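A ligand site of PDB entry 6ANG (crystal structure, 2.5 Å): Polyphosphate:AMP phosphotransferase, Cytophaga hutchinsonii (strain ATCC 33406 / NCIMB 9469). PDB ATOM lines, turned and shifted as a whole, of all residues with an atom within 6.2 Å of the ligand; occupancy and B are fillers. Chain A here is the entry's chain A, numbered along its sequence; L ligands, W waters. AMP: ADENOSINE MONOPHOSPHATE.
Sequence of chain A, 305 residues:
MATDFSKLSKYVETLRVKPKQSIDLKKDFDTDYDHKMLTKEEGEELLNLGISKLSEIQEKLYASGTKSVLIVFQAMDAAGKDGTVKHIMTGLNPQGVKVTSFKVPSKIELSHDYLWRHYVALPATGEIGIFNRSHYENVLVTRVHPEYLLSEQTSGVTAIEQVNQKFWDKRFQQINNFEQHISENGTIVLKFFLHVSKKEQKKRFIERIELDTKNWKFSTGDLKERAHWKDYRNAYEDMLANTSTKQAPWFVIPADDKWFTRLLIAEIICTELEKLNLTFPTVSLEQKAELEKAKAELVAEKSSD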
ATOM      1  N   ASP A  77     -14.723   3.323   5.547  1.00  0.00           N
ATOM      2  CA  ASP A  77     -15.556   4.172   4.713  1.00  0.00           C
ATOM      3  C   ASP A  77     -14.815   4.653   3.497  1.00  0.00           C
ATOM      4  O   ASP A  77     -13.613   4.894   3.535  1.00  0.00           O
ATOM      5  CB  ASP A  77     -16.033   5.390   5.453  1.00  0.00           C
ATOM      6  CG  ASP A  77     -17.050   5.043   6.484  1.00  0.00           C
ATOM      7  OD1 ASP A  77     -17.978   4.270   6.165  1.00  0.00           O
ATOM      8  OD2 ASP A  77     -16.957   5.565   7.629  1.00  0.00           O
ATOM      9  N   LYS A  81     -16.853  -0.064  -1.265  1.00  0.00           N
ATOM     10  CA  LYS A  81     -17.621  -1.269  -0.950  1.00  0.00           C
ATOM     11  C   LYS A  81     -19.030  -1.290  -1.506  1.00  0.00           C
ATOM     12  O   LYS A  81     -19.393  -2.200  -2.228  1.00  0.00           O
ATOM     13  CB  LYS A  81     -17.695  -1.408   0.534  1.00  0.00           C
ATOM     14  CG  LYS A  81     -18.535  -2.563   0.998  1.00  0.00           C
ATOM     15  CD  LYS A  81     -18.293  -2.869   2.466  1.00  0.00           C
ATOM     16  CE  LYS A  81     -18.597  -1.685   3.357  1.00  0.00           C
ATOM     17  NZ  LYS A  81     -20.022  -1.293   3.297  1.00  0.00           N
ATOM     18  N   ASP A  82     -19.789  -0.259  -1.188  1.00  0.00           N
ATOM     19  CA  ASP A  82     -21.156  -0.155  -1.651  1.00  0.00           C
ATOM     20  C   ASP A  82     -21.261  -0.143  -3.140  1.00  0.00           C
ATOM     21  O   ASP A  82     -22.161  -0.745  -3.683  1.00  0.00           O
ATOM     22  CB  ASP A  82     -21.860   1.106  -1.113  1.00  0.00           C
ATOM     23  CG  ASP A  82     -22.366   0.900   0.325  1.00  0.00           C
ATOM     24  OD1 ASP A  82     -21.847   0.061   1.094  1.00  0.00           O
ATOM     25  OD2 ASP A  82     -23.328   1.575   0.682  1.00  0.00           O
ATOM     26  N   SER A 101     -27.705  -5.231   4.030  1.00  0.00           N
ATOM     27  CA  SER A 101     -26.746  -4.283   4.554  1.00  0.00           C
ATOM     28  C   SER A 101     -26.966  -4.123   6.015  1.00  0.00           C
ATOM     29  O   SER A 101     -27.918  -3.477   6.375  1.00  0.00           O
ATOM     30  CB  SER A 101     -26.956  -2.912   3.948  1.00  0.00           C
ATOM     31  OG  SER A 101     -26.393  -2.862   2.675  1.00  0.00           O
ATOM     32  N   PHE A 102     -26.081  -4.605   6.861  1.00  0.00           N
ATOM     33  CA  PHE A 102     -26.344  -4.505   8.285  1.00  0.00           C
ATOM     34  C   PHE A 102     -25.919  -3.166   8.855  1.00  0.00           C
ATOM     35  O   PHE A 102     -24.840  -2.695   8.588  1.00  0.00           O
ATOM     36  CB  PHE A 102     -25.667  -5.620   9.050  1.00  0.00           C
ATOM     37  CG  PHE A 102     -26.234  -6.966   8.755  1.00  0.00           C
ATOM     38  CD1 PHE A 102     -27.272  -7.485   9.503  1.00  0.00           C
ATOM     39  CD2 PHE A 102     -25.690  -7.726   7.742  1.00  0.00           C
ATOM     40  CE1 PHE A 102     -27.765  -8.737   9.231  1.00  0.00           C
ATOM     41  CE2 PHE A 102     -26.192  -8.990   7.453  1.00  0.00           C
ATOM     42  CZ  PHE A 102     -27.227  -9.500   8.205  1.00  0.00           C
ATOM     43  N   LYS A 103     -26.760  -2.599   9.687  1.00  0.00           N
ATOM     44  CA  LYS A 103     -26.488  -1.367  10.331  1.00  0.00           C
ATOM     45  C   LYS A 103     -26.526  -1.496  11.796  1.00  0.00           C
ATOM     46  O   LYS A 103     -26.467  -2.570  12.342  1.00  0.00           O
ATOM     47  CB  LYS A 103     -27.423  -0.290   9.839  1.00  0.00           C
ATOM     48  CG  LYS A 103     -28.880  -0.615   9.765  1.00  0.00           C
ATOM     49  CD  LYS A 103     -29.337  -0.711   8.299  1.00  0.00           C
ATOM     50  CE  LYS A 103     -30.858  -0.960   8.212  1.00  0.00           C
ATOM     51  NZ  LYS A 103     -31.136  -2.081   7.279  1.00  0.00           N
ATOM     52  N   VAL A 104     -26.582  -0.384  12.470  1.00  0.00           N
ATOM     53  CA  VAL A 104     -26.646  -0.438  13.881  1.00  0.00           C
ATOM     54  C   VAL A 104     -27.853  -1.290  14.319  1.00  0.00           C
ATOM     55  O   VAL A 104     -28.937  -1.129  13.838  1.00  0.00           O
ATOM     56  CB  VAL A 104     -26.772   0.975  14.480  1.00  0.00           C
ATOM     57  CG1 VAL A 104     -27.124   0.920  15.961  1.00  0.00           C
ATOM     58  CG2 VAL A 104     -25.429   1.683  14.311  1.00  0.00           C
ATOM     59  N   PRO A 105     -27.632  -2.209  15.223  1.00  0.00           N
ATOM     60  CA  PRO A 105     -28.659  -3.117  15.632  1.00  0.00           C
ATOM     61  C   PRO A 105     -29.848  -2.435  16.268  1.00  0.00           C
ATOM     62  O   PRO A 105     -29.737  -1.443  16.951  1.00  0.00           O
ATOM     63  CB  PRO A 105     -27.949  -3.997  16.642  1.00  0.00           C
ATOM     64  CG  PRO A 105     -26.519  -3.903  16.282  1.00  0.00           C
ATOM     65  CD  PRO A 105     -26.302  -2.565  15.758  1.00  0.00           C
ATOM     66  N   ARG A 117     -28.986 -12.100  14.207  1.00  0.00           N
ATOM     67  CA  ARG A 117     -29.476 -11.436  13.021  1.00  0.00           C
ATOM     68  C   ARG A 117     -28.797 -11.874  11.744  1.00  0.00           C
ATOM     69  O   ARG A 117     -29.419 -11.805  10.688  1.00  0.00           O
ATOM     70  CB  ARG A 117     -29.443  -9.939  13.214  1.00  0.00           C
ATOM     71  CG  ARG A 117     -28.068  -9.292  13.029  1.00  0.00           C
ATOM     72  CD  ARG A 117     -28.180  -7.880  13.534  1.00  0.00           C
ATOM     73  NE  ARG A 117     -26.935  -7.153  13.237  1.00  0.00           N
ATOM     74  CZ  ARG A 117     -26.853  -5.872  12.966  1.00  0.00           C
ATOM     75  NH1 ARG A 117     -27.987  -5.170  12.852  1.00  0.00           N
ATOM     76  NH2 ARG A 117     -25.691  -5.295  12.713  1.00  0.00           N
ATOM     77  N   HIS A 118     -27.566 -12.355  11.805  1.00  0.00           N
ATOM     78  CA  HIS A 118     -26.876 -12.859  10.643  1.00  0.00           C
ATOM     79  C   HIS A 118     -27.324 -14.242  10.279  1.00  0.00           C
ATOM     80  O   HIS A 118     -27.526 -14.538   9.112  1.00  0.00           O
ATOM     81  CB  HIS A 118     -25.369 -12.753  10.829  1.00  0.00           C
ATOM     82  CG  HIS A 118     -24.912 -11.370  11.189  1.00  0.00           C
ATOM     83  ND1 HIS A 118     -24.835 -10.339  10.287  1.00  0.00           N
ATOM     84  CD2 HIS A 118     -24.638 -10.818  12.387  1.00  0.00           C
ATOM     85  CE1 HIS A 118     -24.501  -9.216  10.898  1.00  0.00           C
ATOM     86  NE2 HIS A 118     -24.368  -9.482  12.182  1.00  0.00           N
ATOM     87  N   ARG A 133     -21.613  -5.646   5.032  1.00  0.00           N
ATOM     88  CA  ARG A 133     -21.322  -5.496   6.458  1.00  0.00           C
ATOM     89  C   ARG A 133     -21.889  -6.767   7.120  1.00  0.00           C
ATOM     90  O   ARG A 133     -22.991  -7.185   6.801  1.00  0.00           O
ATOM     91  CB  ARG A 133     -21.840  -4.187   7.010  1.00  0.00           C
ATOM     92  CG  ARG A 133     -20.839  -3.075   6.746  1.00  0.00           C
ATOM     93  CD  ARG A 133     -20.921  -1.989   7.791  1.00  0.00           C
ATOM     94  NE  ARG A 133     -20.651  -0.691   7.196  1.00  0.00           N
ATOM     95  CZ  ARG A 133     -19.450  -0.113   7.181  1.00  0.00           C
ATOM     96  NH1 ARG A 133     -18.420  -0.723   7.735  1.00  0.00           N
ATOM     97  NH2 ARG A 133     -19.299   1.067   6.614  1.00  0.00           N
ATOM     98  N   SER A 134     -21.130  -7.372   8.031  1.00  0.00           N
ATOM     99  CA  SER A 134     -21.509  -8.641   8.573  1.00  0.00           C
ATOM    100  C   SER A 134     -21.356  -8.752  10.041  1.00  0.00           C
ATOM    101  O   SER A 134     -21.310  -7.801  10.709  1.00  0.00           O
ATOM    102  CB  SER A 134     -20.634  -9.658   7.894  1.00  0.00           C
ATOM    103  OG  SER A 134     -19.300  -9.363   8.144  1.00  0.00           O
ATOM    104  N   GLU A 137     -18.552  -7.009  12.092  1.00  0.00           N
ATOM    105  CA  GLU A 137     -18.653  -5.678  12.740  1.00  0.00           C
ATOM    106  C   GLU A 137     -18.482  -5.833  14.235  1.00  0.00           C
ATOM    107  O   GLU A 137     -18.083  -4.924  14.893  1.00  0.00           O
ATOM    108  CB  GLU A 137     -20.043  -5.051  12.508  1.00  0.00           C
ATOM    109  CG  GLU A 137     -20.285  -4.602  11.085  1.00  0.00           C
ATOM    110  CD  GLU A 137     -19.511  -3.363  10.702  1.00  0.00           C
ATOM    111  OE1 GLU A 137     -19.388  -2.438  11.525  1.00  0.00           O
ATOM    112  OE2 GLU A 137     -19.027  -3.329   9.574  1.00  0.00           O
ATOM    113  N   ASN A 138     -18.856  -6.989  14.762  1.00  0.00           N
ATOM    114  CA  ASN A 138     -18.773  -7.250  16.156  1.00  0.00           C
ATOM    115  C   ASN A 138     -17.358  -7.523  16.640  1.00  0.00           C
ATOM    116  O   ASN A 138     -17.143  -7.765  17.807  1.00  0.00           O
ATOM    117  CB  ASN A 138     -19.678  -8.399  16.497  1.00  0.00           C
ATOM    118  CG  ASN A 138     -21.140  -8.101  16.174  1.00  0.00           C
ATOM    119  OD1 ASN A 138     -21.707  -8.704  15.317  1.00  0.00           O
ATOM    120  ND2 ASN A 138     -21.734  -7.189  16.892  1.00  0.00           N
ATOM    121  N   VAL A 141     -15.945  -2.339  14.619  1.00  0.00           N
ATOM    122  CA  VAL A 141     -16.417  -1.105  15.216  1.00  0.00           C
ATOM    123  C   VAL A 141     -16.665  -1.285  16.688  1.00  0.00           C
ATOM    124  O   VAL A 141     -16.559  -0.381  17.427  1.00  0.00           O
ATOM    125  CB  VAL A 141     -17.706  -0.564  14.511  1.00  0.00           C
ATOM    126  CG1 VAL A 141     -18.940  -1.412  14.761  1.00  0.00           C
ATOM    127  CG2 VAL A 141     -18.031   0.802  14.991  1.00  0.00           C
ATOM    128  N   THR A 142     -16.983  -2.483  17.103  1.00  0.00           N
ATOM    129  CA  THR A 142     -17.288  -2.764  18.491  1.00  0.00           C
ATOM    130  C   THR A 142     -15.992  -2.914  19.302  1.00  0.00           C
ATOM    131  O   THR A 142     -16.028  -2.810  20.468  1.00  0.00           O
ATOM    132  CB  THR A 142     -18.116  -4.061  18.465  1.00  0.00           C
ATOM    133  OG1 THR A 142     -19.495  -3.639  18.256  1.00  0.00           O
ATOM    134  CG2 THR A 142     -17.981  -4.785  19.631  1.00  0.00           C
ATOM    135  N   TYR A 148     -20.147   0.294  22.761  1.00  0.00           N
ATOM    136  CA  TYR A 148     -21.321  -0.309  22.170  1.00  0.00           C
ATOM    137  C   TYR A 148     -21.689  -1.633  22.873  1.00  0.00           C
ATOM    138  O   TYR A 148     -22.861  -1.995  22.932  1.00  0.00           O
ATOM    139  CB  TYR A 148     -21.109  -0.590  20.719  1.00  0.00           C
ATOM    140  CG  TYR A 148     -21.079   0.569  19.807  1.00  0.00           C
ATOM    141  CD1 TYR A 148     -22.277   1.111  19.307  1.00  0.00           C
ATOM    142  CD2 TYR A 148     -19.892   1.069  19.330  1.00  0.00           C
ATOM    143  CE1 TYR A 148     -22.267   2.170  18.373  1.00  0.00           C
ATOM    144  CE2 TYR A 148     -19.870   2.134  18.445  1.00  0.00           C
ATOM    145  CZ  TYR A 148     -21.050   2.672  17.962  1.00  0.00           C
ATOM    146  OH  TYR A 148     -20.986   3.708  17.105  1.00  0.00           O
ATOM    147  N   GLU A 152     -25.404  -4.112  24.476  1.00  0.00           N
ATOM    148  CA  GLU A 152     -25.753  -5.469  24.155  1.00  0.00           C
ATOM    149  C   GLU A 152     -26.012  -6.188  25.447  1.00  0.00           C
ATOM    150  O   GLU A 152     -25.109  -6.415  26.204  1.00  0.00           O
ATOM    151  CB  GLU A 152     -24.630  -6.092  23.406  1.00  0.00           C
ATOM    152  CG  GLU A 152     -24.193  -5.292  22.227  1.00  0.00           C
ATOM    153  CD  GLU A 152     -23.157  -6.008  21.374  1.00  0.00           C
ATOM    154  OE1 GLU A 152     -23.149  -7.297  21.254  1.00  0.00           O
ATOM    155  OE2 GLU A 152     -22.313  -5.238  20.853  1.00  0.00           O
ATOM    156  N   GLU A 225     -14.169   8.048  12.420  1.00  0.00           N
ATOM    157  CA  GLU A 225     -13.636   6.750  12.298  1.00  0.00           C
ATOM    158  C   GLU A 225     -12.244   6.832  11.655  1.00  0.00           C
ATOM    159  O   GLU A 225     -11.383   6.018  11.947  1.00  0.00           O
ATOM    160  CB  GLU A 225     -14.570   5.836  11.498  1.00  0.00           C
ATOM    161  CG  GLU A 225     -15.923   5.475  12.193  1.00  0.00           C
ATOM    162  CD  GLU A 225     -15.929   5.583  13.727  1.00  0.00           C
ATOM    163  OE1 GLU A 225     -15.395   4.700  14.437  1.00  0.00           O
ATOM    164  OE2 GLU A 225     -16.475   6.569  14.237  1.00  0.00           O
ATOM    165  N   TYR A 232      -8.547   0.669  14.116  1.00  0.00           N
ATOM    166  CA  TYR A 232      -9.191  -0.190  13.167  1.00  0.00           C
ATOM    167  C   TYR A 232      -8.184  -1.166  12.529  1.00  0.00           C
ATOM    168  O   TYR A 232      -8.526  -2.302  12.277  1.00  0.00           O
ATOM    169  CB  TYR A 232      -9.910   0.620  12.050  1.00  0.00           C
ATOM    170  CG  TYR A 232     -11.306   1.065  12.443  1.00  0.00           C
ATOM    171  CD1 TYR A 232     -12.358   0.159  12.447  1.00  0.00           C
ATOM    172  CD2 TYR A 232     -11.577   2.370  12.785  1.00  0.00           C
ATOM    173  CE1 TYR A 232     -13.620   0.498  12.844  1.00  0.00           C
ATOM    174  CE2 TYR A 232     -12.852   2.743  13.147  1.00  0.00           C
ATOM    175  CZ  TYR A 232     -13.876   1.792  13.173  1.00  0.00           C
ATOM    176  OH  TYR A 232     -15.167   2.141  13.526  1.00  0.00           O
HETATM  177  P   AMP L   1     -24.310   3.042   6.902  1.00  0.00           P
HETATM  178  O1P AMP L   1     -24.155   4.522   7.227  1.00  0.00           O
HETATM  179  O2P AMP L   1     -25.545   2.669   6.122  1.00  0.00           O
HETATM  180  O3P AMP L   1     -23.004   2.341   6.512  1.00  0.00           O
HETATM  181  O5' AMP L   1     -24.685   2.455   8.351  1.00  0.00           O
HETATM  182  C5' AMP L   1     -24.045   1.297   8.888  1.00  0.00           C
HETATM  183  C4' AMP L   1     -23.330   1.633  10.191  1.00  0.00           C
HETATM  184  O4' AMP L   1     -23.754   0.731  11.222  1.00  0.00           O
HETATM  185  C3' AMP L   1     -21.816   1.537  10.088  1.00  0.00           C
HETATM  186  O3' AMP L   1     -21.178   2.566  10.813  1.00  0.00           O
HETATM  187  C2' AMP L   1     -21.508   0.289  10.865  1.00  0.00           C
HETATM  188  O2' AMP L   1     -20.175   0.194  11.398  1.00  0.00           O
HETATM  189  C1' AMP L   1     -22.656   0.254  11.927  1.00  0.00           C
HETATM  190  N9  AMP L   1     -22.884  -1.142  12.391  1.00  0.00           N
HETATM  191  C8  AMP L   1     -23.090  -2.232  11.641  1.00  0.00           C
HETATM  192  N7  AMP L   1     -23.139  -3.337  12.421  1.00  0.00           N
HETATM  193  C5  AMP L   1     -22.940  -2.951  13.686  1.00  0.00           C
HETATM  194  C6  AMP L   1     -22.919  -3.609  14.977  1.00  0.00           C
HETATM  195  N6  AMP L   1     -23.085  -4.956  15.072  1.00  0.00           N
HETATM  196  N1  AMP L   1     -22.768  -2.870  16.080  1.00  0.00           N
HETATM  197  C2  AMP L   1     -22.587  -1.522  16.018  1.00  0.00           C
HETATM  198  N3  AMP L   1     -22.598  -0.848  14.847  1.00  0.00           N
HETATM  199  C4  AMP L   1     -22.779  -1.521  13.661  1.00  0.00           C
HETATM  200  O   HOH W   1     -26.429   2.634  11.202  1.00  0.00           O
HETATM  201  O   HOH W   2     -23.394  -3.802  18.628  1.00  0.00           O
HETATM  202  O   HOH W   3     -23.077  -6.916  12.730  1.00  0.00           O
HETATM  203  O   HOH W   4     -24.427  -6.357  17.965  1.00  0.00           O
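The guanidinium group of Arg 117 lies within hydrogen-bond range of a nitrogen (N7) of the ligand (3.2 Å). OE1 of Glu 137 sits at hydrogen-bond distance from O2' of the ligand, 2.8 Å away. The backbone NH (N) of Val 104 is in hydrogen-bond range of an oxygen (O4') of the ligand. NE of Arg 133 is in salt-bridge range of O3P of the ligand (3.9 Å). The side-chain amide nitrogen (ND2) of Asn 138 sits close to a nitrogen (N6) of the ligand (3.2 Å).
NH2 of Arg 117 is in hydrogen-bond range of O of Lys 103 (2.9 Å). The side-chain carboxylate (OE2) of Glu 137 is in salt-bridge range of the guanidinium group (NH1) of Arg 133 (3.2 Å). N of Thr 142 lies within hydrogen-bond range of O of Glu 137 (3.5 Å). The side-chain carboxylate (OD1) of Asp 77 is in salt-bridge range of the guanidinium group (NH2) of Arg 133 (3.5 Å).
N7 of the ligand lies close to O of Lys 103 (3.4 Å). O of Phe 102 touches C8 of the ligand, 3.5 Å away. Pro 105 touches the ligand. Val 141 touches the ligand. Hydrophobic or aromatic side chains that line the ligand: Val 104, Pro 105 and Val 141. Within 4 Å of the ligand: Phe 102, Lys 103, Val 104, Pro 105, Arg 117, Arg 133, Glu 137, Asn 138 and Val 141. The nearest printed residue that does not touch the ligand is Thr 142 (4.005 Å).
Water W2 lies within hydrogen-bond range of N1 of the ligand and OE2 of Glu 152. Water W3 lies within hydrogen-bond range of the backbone carbonyl oxygen of Ser 134, a ring nitrogen (NE2) of His 118, a nitrogen (N6) of the ligand, the guanidinium group of Arg 117 and the side-chain amide oxygen of Asn 138. Water W1 lies within hydrogen-bond range of N of Val 104 (3.3 Å) and O4' of the ligand (3.3 Å). Water W4 bridges ND2 of Asn 138 and N6 of the ligand.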
